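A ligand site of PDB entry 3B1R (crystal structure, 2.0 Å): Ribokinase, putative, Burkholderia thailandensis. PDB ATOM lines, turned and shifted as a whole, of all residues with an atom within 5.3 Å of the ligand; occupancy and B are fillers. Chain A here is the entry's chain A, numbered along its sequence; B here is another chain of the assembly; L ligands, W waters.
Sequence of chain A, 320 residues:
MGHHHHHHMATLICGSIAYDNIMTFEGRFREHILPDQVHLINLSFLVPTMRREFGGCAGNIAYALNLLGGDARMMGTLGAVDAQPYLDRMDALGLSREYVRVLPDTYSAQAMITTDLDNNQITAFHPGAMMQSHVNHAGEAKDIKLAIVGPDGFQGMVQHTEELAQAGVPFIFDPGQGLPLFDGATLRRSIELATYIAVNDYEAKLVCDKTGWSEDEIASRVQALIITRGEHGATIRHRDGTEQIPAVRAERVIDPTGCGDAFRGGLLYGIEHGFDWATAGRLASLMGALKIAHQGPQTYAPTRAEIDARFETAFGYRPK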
ATOM      1  N   LEU A 117      -6.502   4.520  -0.564  1.00  0.00           N
ATOM      2  CA  LEU A 117      -7.291   4.147  -1.742  1.00  0.00           C
ATOM      3  C   LEU A 117      -8.608   3.462  -1.390  1.00  0.00           C
ATOM      4  O   LEU A 117      -9.400   3.138  -2.281  1.00  0.00           O
ATOM      5  CB  LEU A 117      -6.450   3.308  -2.719  1.00  0.00           C
ATOM      6  CG  LEU A 117      -5.229   4.053  -3.284  1.00  0.00           C
ATOM      7  CD1 LEU A 117      -4.361   3.127  -4.125  1.00  0.00           C
ATOM      8  CD2 LEU A 117      -5.659   5.294  -4.096  1.00  0.00           C
ATOM      9  N   ASP A 118      -8.830   3.255  -0.099  1.00  0.00           N
ATOM     10  CA  ASP A 118     -10.094   2.762   0.438  1.00  0.00           C
ATOM     11  C   ASP A 118     -10.999   3.897   0.885  1.00  0.00           C
ATOM     12  O   ASP A 118     -12.042   3.640   1.503  1.00  0.00           O
ATOM     13  CB  ASP A 118      -9.858   1.837   1.633  1.00  0.00           C
ATOM     14  CG  ASP A 118      -9.803   0.384   1.250  1.00  0.00           C
ATOM     15  OD1 ASP A 118      -9.730   0.100   0.049  1.00  0.00           O
ATOM     16  OD2 ASP A 118      -9.814  -0.470   2.170  1.00  0.00           O
ATOM     17  N   ASN A 119     -10.579   5.133   0.625  1.00  0.00           N
ATOM     18  CA  ASN A 119     -11.336   6.324   1.043  1.00  0.00           C
ATOM     19  C   ASN A 119     -11.514   6.469   2.569  1.00  0.00           C
ATOM     20  O   ASN A 119     -12.498   7.061   3.053  1.00  0.00           O
ATOM     21  CB  ASN A 119     -12.683   6.379   0.325  1.00  0.00           C
ATOM     22  CG  ASN A 119     -13.199   7.786   0.163  1.00  0.00           C
ATOM     23  OD1 ASN A 119     -12.491   8.751   0.413  1.00  0.00           O
ATOM     24  ND2 ASN A 119     -14.444   7.908  -0.232  1.00  0.00           N
ATOM     25  N   ASN A 200     -22.114   6.698   3.335  1.00  0.00           N
ATOM     26  CA  ASN A 200     -21.241   5.563   3.047  1.00  0.00           C
ATOM     27  C   ASN A 200     -21.457   4.545   4.172  1.00  0.00           C
ATOM     28  O   ASN A 200     -22.121   4.876   5.152  1.00  0.00           O
ATOM     29  CB  ASN A 200     -19.752   5.968   2.829  1.00  0.00           C
ATOM     30  CG  ASN A 200     -19.044   6.438   4.106  1.00  0.00           C
ATOM     31  OD1 ASN A 200     -19.334   5.970   5.212  1.00  0.00           O
ATOM     32  ND2 ASN A 200     -18.079   7.350   3.940  1.00  0.00           N
ATOM     33  N   THR A 228     -23.304   3.784   0.217  1.00  0.00           N
ATOM     34  CA  THR A 228     -22.215   3.547  -0.725  1.00  0.00           C
ATOM     35  C   THR A 228     -21.120   2.767  -0.021  1.00  0.00           C
ATOM     36  O   THR A 228     -20.864   2.968   1.153  1.00  0.00           O
ATOM     37  CB  THR A 228     -21.624   4.866  -1.326  1.00  0.00           C
ATOM     38  OG1 THR A 228     -20.910   5.576  -0.321  1.00  0.00           O
ATOM     39  CG2 THR A 228     -22.714   5.758  -1.884  1.00  0.00           C
ATOM     40  N   ARG A 229     -20.498   1.847  -0.769  1.00  0.00           N
ATOM     41  CA  ARG A 229     -19.487   0.949  -0.251  1.00  0.00           C
ATOM     42  C   ARG A 229     -18.305   0.878  -1.236  1.00  0.00           C
ATOM     43  O   ARG A 229     -17.916  -0.219  -1.675  1.00  0.00           O
ATOM     44  CB  ARG A 229     -20.066  -0.457  -0.016  1.00  0.00           C
ATOM     45  CG  ARG A 229     -21.493  -0.499   0.571  1.00  0.00           C
ATOM     46  CD  ARG A 229     -21.895  -1.905   0.966  1.00  0.00           C
ATOM     47  NE  ARG A 229     -23.325  -2.040   1.239  1.00  0.00           N
ATOM     48  CZ  ARG A 229     -23.887  -1.909   2.437  1.00  0.00           C
ATOM     49  NH1 ARG A 229     -23.139  -1.623   3.496  1.00  0.00           N
ATOM     50  NH2 ARG A 229     -25.194  -2.032   2.585  1.00  0.00           N
ATOM     51  N   GLY A 230     -17.757   2.036  -1.586  1.00  0.00           N
ATOM     52  CA  GLY A 230     -16.561   2.098  -2.419  1.00  0.00           C
ATOM     53  C   GLY A 230     -16.619   1.219  -3.657  1.00  0.00           C
ATOM     54  O   GLY A 230     -17.599   1.234  -4.403  1.00  0.00           O
ATOM     55  N   GLU A 231     -15.581   0.418  -3.888  1.00  0.00           N
ATOM     56  CA  GLU A 231     -15.511  -0.398  -5.101  1.00  0.00           C
ATOM     57  C   GLU A 231     -16.610  -1.458  -5.184  1.00  0.00           C
ATOM     58  O   GLU A 231     -16.786  -2.101  -6.214  1.00  0.00           O
ATOM     59  CB  GLU A 231     -14.121  -1.018  -5.277  1.00  0.00           C
ATOM     60  CG  GLU A 231     -13.747  -2.086  -4.271  1.00  0.00           C
ATOM     61  CD  GLU A 231     -12.494  -2.862  -4.694  1.00  0.00           C
ATOM     62  OE1 GLU A 231     -12.513  -3.488  -5.777  1.00  0.00           O
ATOM     63  OE2 GLU A 231     -11.507  -2.836  -3.943  1.00  0.00           O
ATOM     64  N   GLY A 233     -19.785  -0.783  -4.890  1.00  0.00           N
ATOM     65  CA  GLY A 233     -20.989  -0.096  -5.371  1.00  0.00           C
ATOM     66  C   GLY A 233     -21.811   0.561  -4.270  1.00  0.00           C
ATOM     67  O   GLY A 233     -21.264   1.159  -3.334  1.00  0.00           O
ATOM     68  N   ALA A 234     -23.121   0.447  -4.398  1.00  0.00           N
ATOM     69  CA  ALA A 234     -24.073   1.064  -3.476  1.00  0.00           C
ATOM     70  C   ALA A 234     -25.371   0.265  -3.348  1.00  0.00           C
ATOM     71  O   ALA A 234     -25.731  -0.516  -4.228  1.00  0.00           O
ATOM     72  CB  ALA A 234     -24.378   2.513  -3.906  1.00  0.00           C
ATOM     73  N   PRO A 246     -24.061  -1.430  -9.124  1.00  0.00           N
ATOM     74  CA  PRO A 246     -22.698  -1.867  -9.386  1.00  0.00           C
ATOM     75  C   PRO A 246     -21.723  -0.689  -9.319  1.00  0.00           C
ATOM     76  O   PRO A 246     -22.127   0.476  -9.463  1.00  0.00           O
ATOM     77  CB  PRO A 246     -22.777  -2.386 -10.824  1.00  0.00           C
ATOM     78  CG  PRO A 246     -23.805  -1.507 -11.466  1.00  0.00           C
ATOM     79  CD  PRO A 246     -24.836  -1.250 -10.386  1.00  0.00           C
ATOM     80  N   ALA A 247     -20.451  -1.000  -9.091  1.00  0.00           N
ATOM     81  CA  ALA A 247     -19.395  -0.008  -9.305  1.00  0.00           C
ATOM     82  C   ALA A 247     -18.962  -0.079 -10.767  1.00  0.00           C
ATOM     83  O   ALA A 247     -18.778  -1.171 -11.331  1.00  0.00           O
ATOM     84  CB  ALA A 247     -18.210  -0.263  -8.387  1.00  0.00           C
ATOM     85  N   VAL A 248     -18.834   1.082 -11.407  1.00  0.00           N
ATOM     86  CA  VAL A 248     -18.201   1.142 -12.716  1.00  0.00           C
ATOM     87  C   VAL A 248     -16.702   0.978 -12.472  1.00  0.00           C
ATOM     88  O   VAL A 248     -16.093   1.779 -11.755  1.00  0.00           O
ATOM     89  CB  VAL A 248     -18.526   2.473 -13.451  1.00  0.00           C
ATOM     90  CG1 VAL A 248     -17.881   2.525 -14.832  1.00  0.00           C
ATOM     91  CG2 VAL A 248     -20.025   2.663 -13.563  1.00  0.00           C
ATOM     92  N   ARG A 249     -16.109  -0.086 -13.031  1.00  0.00           N
ATOM     93  CA  ARG A 249     -14.677  -0.344 -12.828  1.00  0.00           C
ATOM     94  C   ARG A 249     -13.846   0.884 -13.204  1.00  0.00           C
ATOM     95  O   ARG A 249     -14.066   1.504 -14.256  1.00  0.00           O
ATOM     96  CB  ARG A 249     -14.218  -1.583 -13.612  1.00  0.00           C
ATOM     97  CG  ARG A 249     -12.943  -2.203 -13.058  1.00  0.00           C
ATOM     98  CD  ARG A 249     -12.365  -3.254 -13.998  1.00  0.00           C
ATOM     99  NE  ARG A 249     -10.981  -2.912 -14.317  1.00  0.00           N
ATOM    100  CZ  ARG A 249      -9.943  -3.136 -13.520  1.00  0.00           C
ATOM    101  NH1 ARG A 249     -10.118  -3.742 -12.350  1.00  0.00           N
ATOM    102  NH2 ARG A 249      -8.729  -2.767 -13.904  1.00  0.00           N
ATOM    103  N   ALA A 250     -12.925   1.262 -12.332  1.00  0.00           N
ATOM    104  CA  ALA A 250     -12.195   2.512 -12.485  1.00  0.00           C
ATOM    105  C   ALA A 250     -11.083   2.369 -13.510  1.00  0.00           C
ATOM    106  O   ALA A 250     -10.360   1.384 -13.482  1.00  0.00           O
ATOM    107  CB  ALA A 250     -11.622   2.950 -11.143  1.00  0.00           C
ATOM    108  N   VAL A 253      -7.191   3.924 -10.035  1.00  0.00           N
ATOM    109  CA  VAL A 253      -7.545   4.480  -8.739  1.00  0.00           C
ATOM    110  C   VAL A 253      -6.407   5.385  -8.255  1.00  0.00           C
ATOM    111  O   VAL A 253      -5.305   4.910  -7.927  1.00  0.00           O
ATOM    112  CB  VAL A 253      -7.865   3.367  -7.714  1.00  0.00           C
ATOM    113  CG1 VAL A 253      -8.308   3.947  -6.377  1.00  0.00           C
ATOM    114  CG2 VAL A 253      -8.940   2.421  -8.257  1.00  0.00           C
ATOM    115  N   PRO A 256      -9.801   8.745  -3.899  1.00  0.00           N
ATOM    116  CA  PRO A 256     -11.244   8.657  -3.723  1.00  0.00           C
ATOM    117  C   PRO A 256     -11.872   9.883  -3.046  1.00  0.00           C
ATOM    118  O   PRO A 256     -13.094   9.993  -3.041  1.00  0.00           O
ATOM    119  CB  PRO A 256     -11.440   7.386  -2.880  1.00  0.00           C
ATOM    120  CG  PRO A 256     -10.090   6.881  -2.545  1.00  0.00           C
ATOM    121  CD  PRO A 256      -9.103   7.968  -2.864  1.00  0.00           C
ATOM    122  N   CYS A 259     -15.432  11.192  -3.926  1.00  0.00           N
ATOM    123  CA  CYS A 259     -16.266  10.170  -4.590  1.00  0.00           C
ATOM    124  C   CYS A 259     -17.696  10.169  -4.071  1.00  0.00           C
ATOM    125  O   CYS A 259     -18.640  10.008  -4.845  1.00  0.00           O
ATOM    126  CB  CYS A 259     -15.661   8.767  -4.492  1.00  0.00           C
ATOM    127  SG  CYS A 259     -14.311   8.481  -5.666  1.00  0.00           S
ATOM    128  N   GLY A 260     -17.850  10.350  -2.758  1.00  0.00           N
ATOM    129  CA  GLY A 260     -19.191  10.464  -2.165  1.00  0.00           C
ATOM    130  C   GLY A 260     -19.968  11.581  -2.840  1.00  0.00           C
ATOM    131  O   GLY A 260     -21.129  11.416  -3.213  1.00  0.00           O
ATOM    132  N   PHE A 263     -20.936  11.086  -6.594  1.00  0.00           N
ATOM    133  CA  PHE A 263     -22.026  10.095  -6.586  1.00  0.00           C
ATOM    134  C   PHE A 263     -23.343  10.804  -6.273  1.00  0.00           C
ATOM    135  O   PHE A 263     -24.356  10.539  -6.931  1.00  0.00           O
ATOM    136  CB  PHE A 263     -21.728   9.016  -5.533  1.00  0.00           C
ATOM    137  CG  PHE A 263     -22.749   7.898  -5.472  1.00  0.00           C
ATOM    138  CD1 PHE A 263     -22.530   6.708  -6.157  1.00  0.00           C
ATOM    139  CD2 PHE A 263     -23.902   8.024  -4.703  1.00  0.00           C
ATOM    140  CE1 PHE A 263     -23.455   5.666  -6.102  1.00  0.00           C
ATOM    141  CE2 PHE A 263     -24.832   6.986  -4.635  1.00  0.00           C
ATOM    142  CZ  PHE A 263     -24.605   5.801  -5.335  1.00  0.00           C
ATOM    143  N   ALA A 284     -24.909   7.790 -10.714  1.00  0.00           N
ATOM    144  CA  ALA A 284     -24.172   8.214  -9.514  1.00  0.00           C
ATOM    145  C   ALA A 284     -22.869   7.469  -9.387  1.00  0.00           C
ATOM    146  O   ALA A 284     -21.817   8.057  -9.077  1.00  0.00           O
ATOM    147  CB  ALA A 284     -25.018   7.982  -8.271  1.00  0.00           C
ATOM    148  N   SER A 285     -22.940   6.156  -9.629  1.00  0.00           N
ATOM    149  CA  SER A 285     -21.801   5.277  -9.516  1.00  0.00           C
ATOM    150  C   SER A 285     -20.777   5.595 -10.594  1.00  0.00           C
ATOM    151  O   SER A 285     -19.560   5.538 -10.345  1.00  0.00           O
ATOM    152  CB  SER A 285     -22.250   3.831  -9.605  1.00  0.00           C
ATOM    153  OG  SER A 285     -21.138   2.974  -9.470  1.00  0.00           O
ATOM    154  N   LEU A 286     -21.260   5.946 -11.793  1.00  0.00           N
ATOM    155  CA  LEU A 286     -20.373   6.395 -12.847  1.00  0.00           C
ATOM    156  C   LEU A 286     -19.579   7.611 -12.386  1.00  0.00           C
ATOM    157  O   LEU A 286     -18.363   7.595 -12.460  1.00  0.00           O
ATOM    158  CB  LEU A 286     -21.123   6.687 -14.149  1.00  0.00           C
ATOM    159  CG  LEU A 286     -20.214   7.108 -15.312  1.00  0.00           C
ATOM    160  CD1 LEU A 286     -19.117   6.079 -15.579  1.00  0.00           C
ATOM    161  CD2 LEU A 286     -21.034   7.345 -16.567  1.00  0.00           C
ATOM    162  N   GLY A 288     -18.806   8.601  -9.521  1.00  0.00           N
ATOM    163  CA  GLY A 288     -17.866   8.039  -8.547  1.00  0.00           C
ATOM    164  C   GLY A 288     -16.629   7.405  -9.181  1.00  0.00           C
ATOM    165  O   GLY A 288     -15.518   7.644  -8.723  1.00  0.00           O
ATOM    166  N   ALA A 289     -16.826   6.607 -10.225  1.00  0.00           N
ATOM    167  CA  ALA A 289     -15.711   5.980 -10.957  1.00  0.00           C
ATOM    168  C   ALA A 289     -14.841   6.967 -11.736  1.00  0.00           C
ATOM    169  O   ALA A 289     -13.607   6.831 -11.745  1.00  0.00           O
ATOM    170  CB  ALA A 289     -16.216   4.864 -11.870  1.00  0.00           C
ATOM    171  N   ILE A 292     -12.528   9.129  -9.224  1.00  0.00           N
ATOM    172  CA  ILE A 292     -11.462   8.372  -8.552  1.00  0.00           C
ATOM    173  C   ILE A 292     -10.187   8.268  -9.402  1.00  0.00           C
ATOM    174  O   ILE A 292      -9.134   7.885  -8.901  1.00  0.00           O
ATOM    175  CB  ILE A 292     -11.945   6.956  -8.119  1.00  0.00           C
ATOM    176  CG1 ILE A 292     -11.113   6.432  -6.952  1.00  0.00           C
ATOM    177  CG2 ILE A 292     -11.908   5.964  -9.306  1.00  0.00           C
ATOM    178  CD1 ILE A 292     -11.785   5.282  -6.212  1.00  0.00           C
ATOM    179  N   HIS B  39     -15.323   0.812   4.304  1.00  0.00           N
ATOM    180  CA  HIS B  39     -14.529   1.914   4.838  1.00  0.00           C
ATOM    181  C   HIS B  39     -14.158   1.615   6.286  1.00  0.00           C
ATOM    182  O   HIS B  39     -15.028   1.562   7.165  1.00  0.00           O
ATOM    183  CB  HIS B  39     -15.304   3.218   4.783  1.00  0.00           C
ATOM    184  CG  HIS B  39     -15.788   3.577   3.417  1.00  0.00           C
ATOM    185  ND1 HIS B  39     -17.058   3.295   2.981  1.00  0.00           N
ATOM    186  CD2 HIS B  39     -15.164   4.208   2.399  1.00  0.00           C
ATOM    187  CE1 HIS B  39     -17.201   3.736   1.738  1.00  0.00           C
ATOM    188  NE2 HIS B  39     -16.066   4.302   1.368  1.00  0.00           N
HETATM  189  P1  LIG L   1     -17.508   5.937  -1.316  1.00  0.00           P
HETATM  190  O1  LIG L   1     -17.848   7.319  -0.806  1.00  0.00           O
HETATM  191  O2  LIG L   1     -16.049   5.605  -1.120  1.00  0.00           O
HETATM  192  O3  LIG L   1     -18.478   4.874  -0.850  1.00  0.00           O
HETATM  193  O4  LIG L   1     -17.669   6.030  -2.895  1.00  0.00           O
HETATM  194  C1  LIG L   1     -18.860   6.552  -3.439  1.00  0.00           C
HETATM  195  C2  LIG L   1     -19.146   5.874  -4.758  1.00  0.00           C
HETATM  196  O5  LIG L   1     -18.117   6.242  -5.686  1.00  0.00           O
HETATM  197  C3  LIG L   1     -19.178   4.348  -4.730  1.00  0.00           C
HETATM  198  O6  LIG L   1     -20.438   3.770  -4.345  1.00  0.00           O
HETATM  199  C4  LIG L   1     -18.831   4.063  -6.172  1.00  0.00           C
HETATM  200  O7  LIG L   1     -19.951   4.271  -7.062  1.00  0.00           O
HETATM  201  C5  LIG L   1     -17.793   5.111  -6.502  1.00  0.00           C
HETATM  202  N1  LIG L   1     -16.502   4.499  -6.100  1.00  0.00           N
HETATM  203  C6  LIG L   1     -15.839   4.643  -4.927  1.00  0.00           C
HETATM  204  N2  LIG L   1     -14.703   3.889  -4.930  1.00  0.00           N
HETATM  205  C7  LIG L   1     -14.647   3.243  -6.114  1.00  0.00           C
HETATM  206  C8  LIG L   1     -13.718   2.292  -6.772  1.00  0.00           C
HETATM  207  N3  LIG L   1     -12.600   1.872  -6.145  1.00  0.00           N
HETATM  208  N4  LIG L   1     -14.037   1.853  -8.012  1.00  0.00           N
HETATM  209  C9  LIG L   1     -15.150   2.255  -8.663  1.00  0.00           C
HETATM  210  N5  LIG L   1     -16.029   3.127  -8.112  1.00  0.00           N
HETATM  211  C10 LIG L   1     -15.832   3.645  -6.874  1.00  0.00           C
HETATM  212  O   HOH W   1     -17.118   8.338   1.601  1.00  0.00           O
HETATM  213  O   HOH W   2     -10.923  -0.186  -6.978  1.00  0.00           O
HETATM  214  O   HOH W   3     -20.390   8.020  -0.236  1.00  0.00           O
HETATM  215  O   HOH W   4     -12.801   0.163  -9.679  1.00  0.00           O
HETATM  216  O   HOH W   5     -18.396   3.403  -9.404  1.00  0.00           O
HETATM  217  O   HOH W   6     -15.956  10.242  -0.799  1.00  0.00           O
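O3 of the ligand lies within hydrogen-bond range of OG1 of Thr 228, 2.6 Å away. O2 of the ligand is in hydrogen-bond range of NE2 of His 39 of chain B (2.8 Å). The backbone carbonyl oxygen (O) of Gly 233 is in hydrogen-bond range of an oxygen (O6) of the ligand (2.9 Å). An oxygen (O2) of the ligand is in hydrogen-bond range of the side-chain amide nitrogen (ND2) of Asn 119. OG of Ser 285 sits at hydrogen-bond distance from O7 of the ligand (3.0 Å). The backbone NH (N) of Gly 230 is in hydrogen-bond range of an oxygen (O3) of the ligand.
The backbone carbonyl oxygen (O) of Pro 246 sits at hydrogen-bond distance from the side-chain hydroxyl (OG) of Ser 285, at 2.7 Å. O of Gly 288 sits at hydrogen-bond distance from SG of Cys 259, 3.4 Å away. The side-chain sulfur (SG) of Cys 259 sits close to the backbone carbonyl oxygen (O) of Pro 256, 3.3 Å away.
Merely in contact with the ligand: Val 248 (3.3 Å), Glu 231 (3.4 Å), Gly 288 (3.4 Å), Ile 292 (3.5 Å), Gly 260 (3.6 Å), Arg 229 (3.6 Å), Phe 263 (3.7 Å), Cys 259 (3.7 Å) and Ala 247 (3.97 Å). Hydrophobic or aromatic side chains within 4 Å of the ligand: Ala 247, Phe 263, Ile 292 and His 39 of chain B. Of the 27 residues printed, 15 come within 4 Å of the ligand.
Water W4 lies within hydrogen-bond range of a nitrogen (N4) of the ligand (2.7 Å) and the backbone NH (N) of Ala 250 (2.9 Å). Water W3 lies within hydrogen-bond range of the side-chain hydroxyl of Thr 228 (2.5 Å) and an oxygen (O1) of the ligand (2.7 Å). Water W5 lies within hydrogen-bond range of O of Ser 285, N5 of the ligand and N of Val 248. Water W1 lies within hydrogen-bond range of O1 of the ligand, ND2 of Asn 200 and ND2 of Asn 119.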
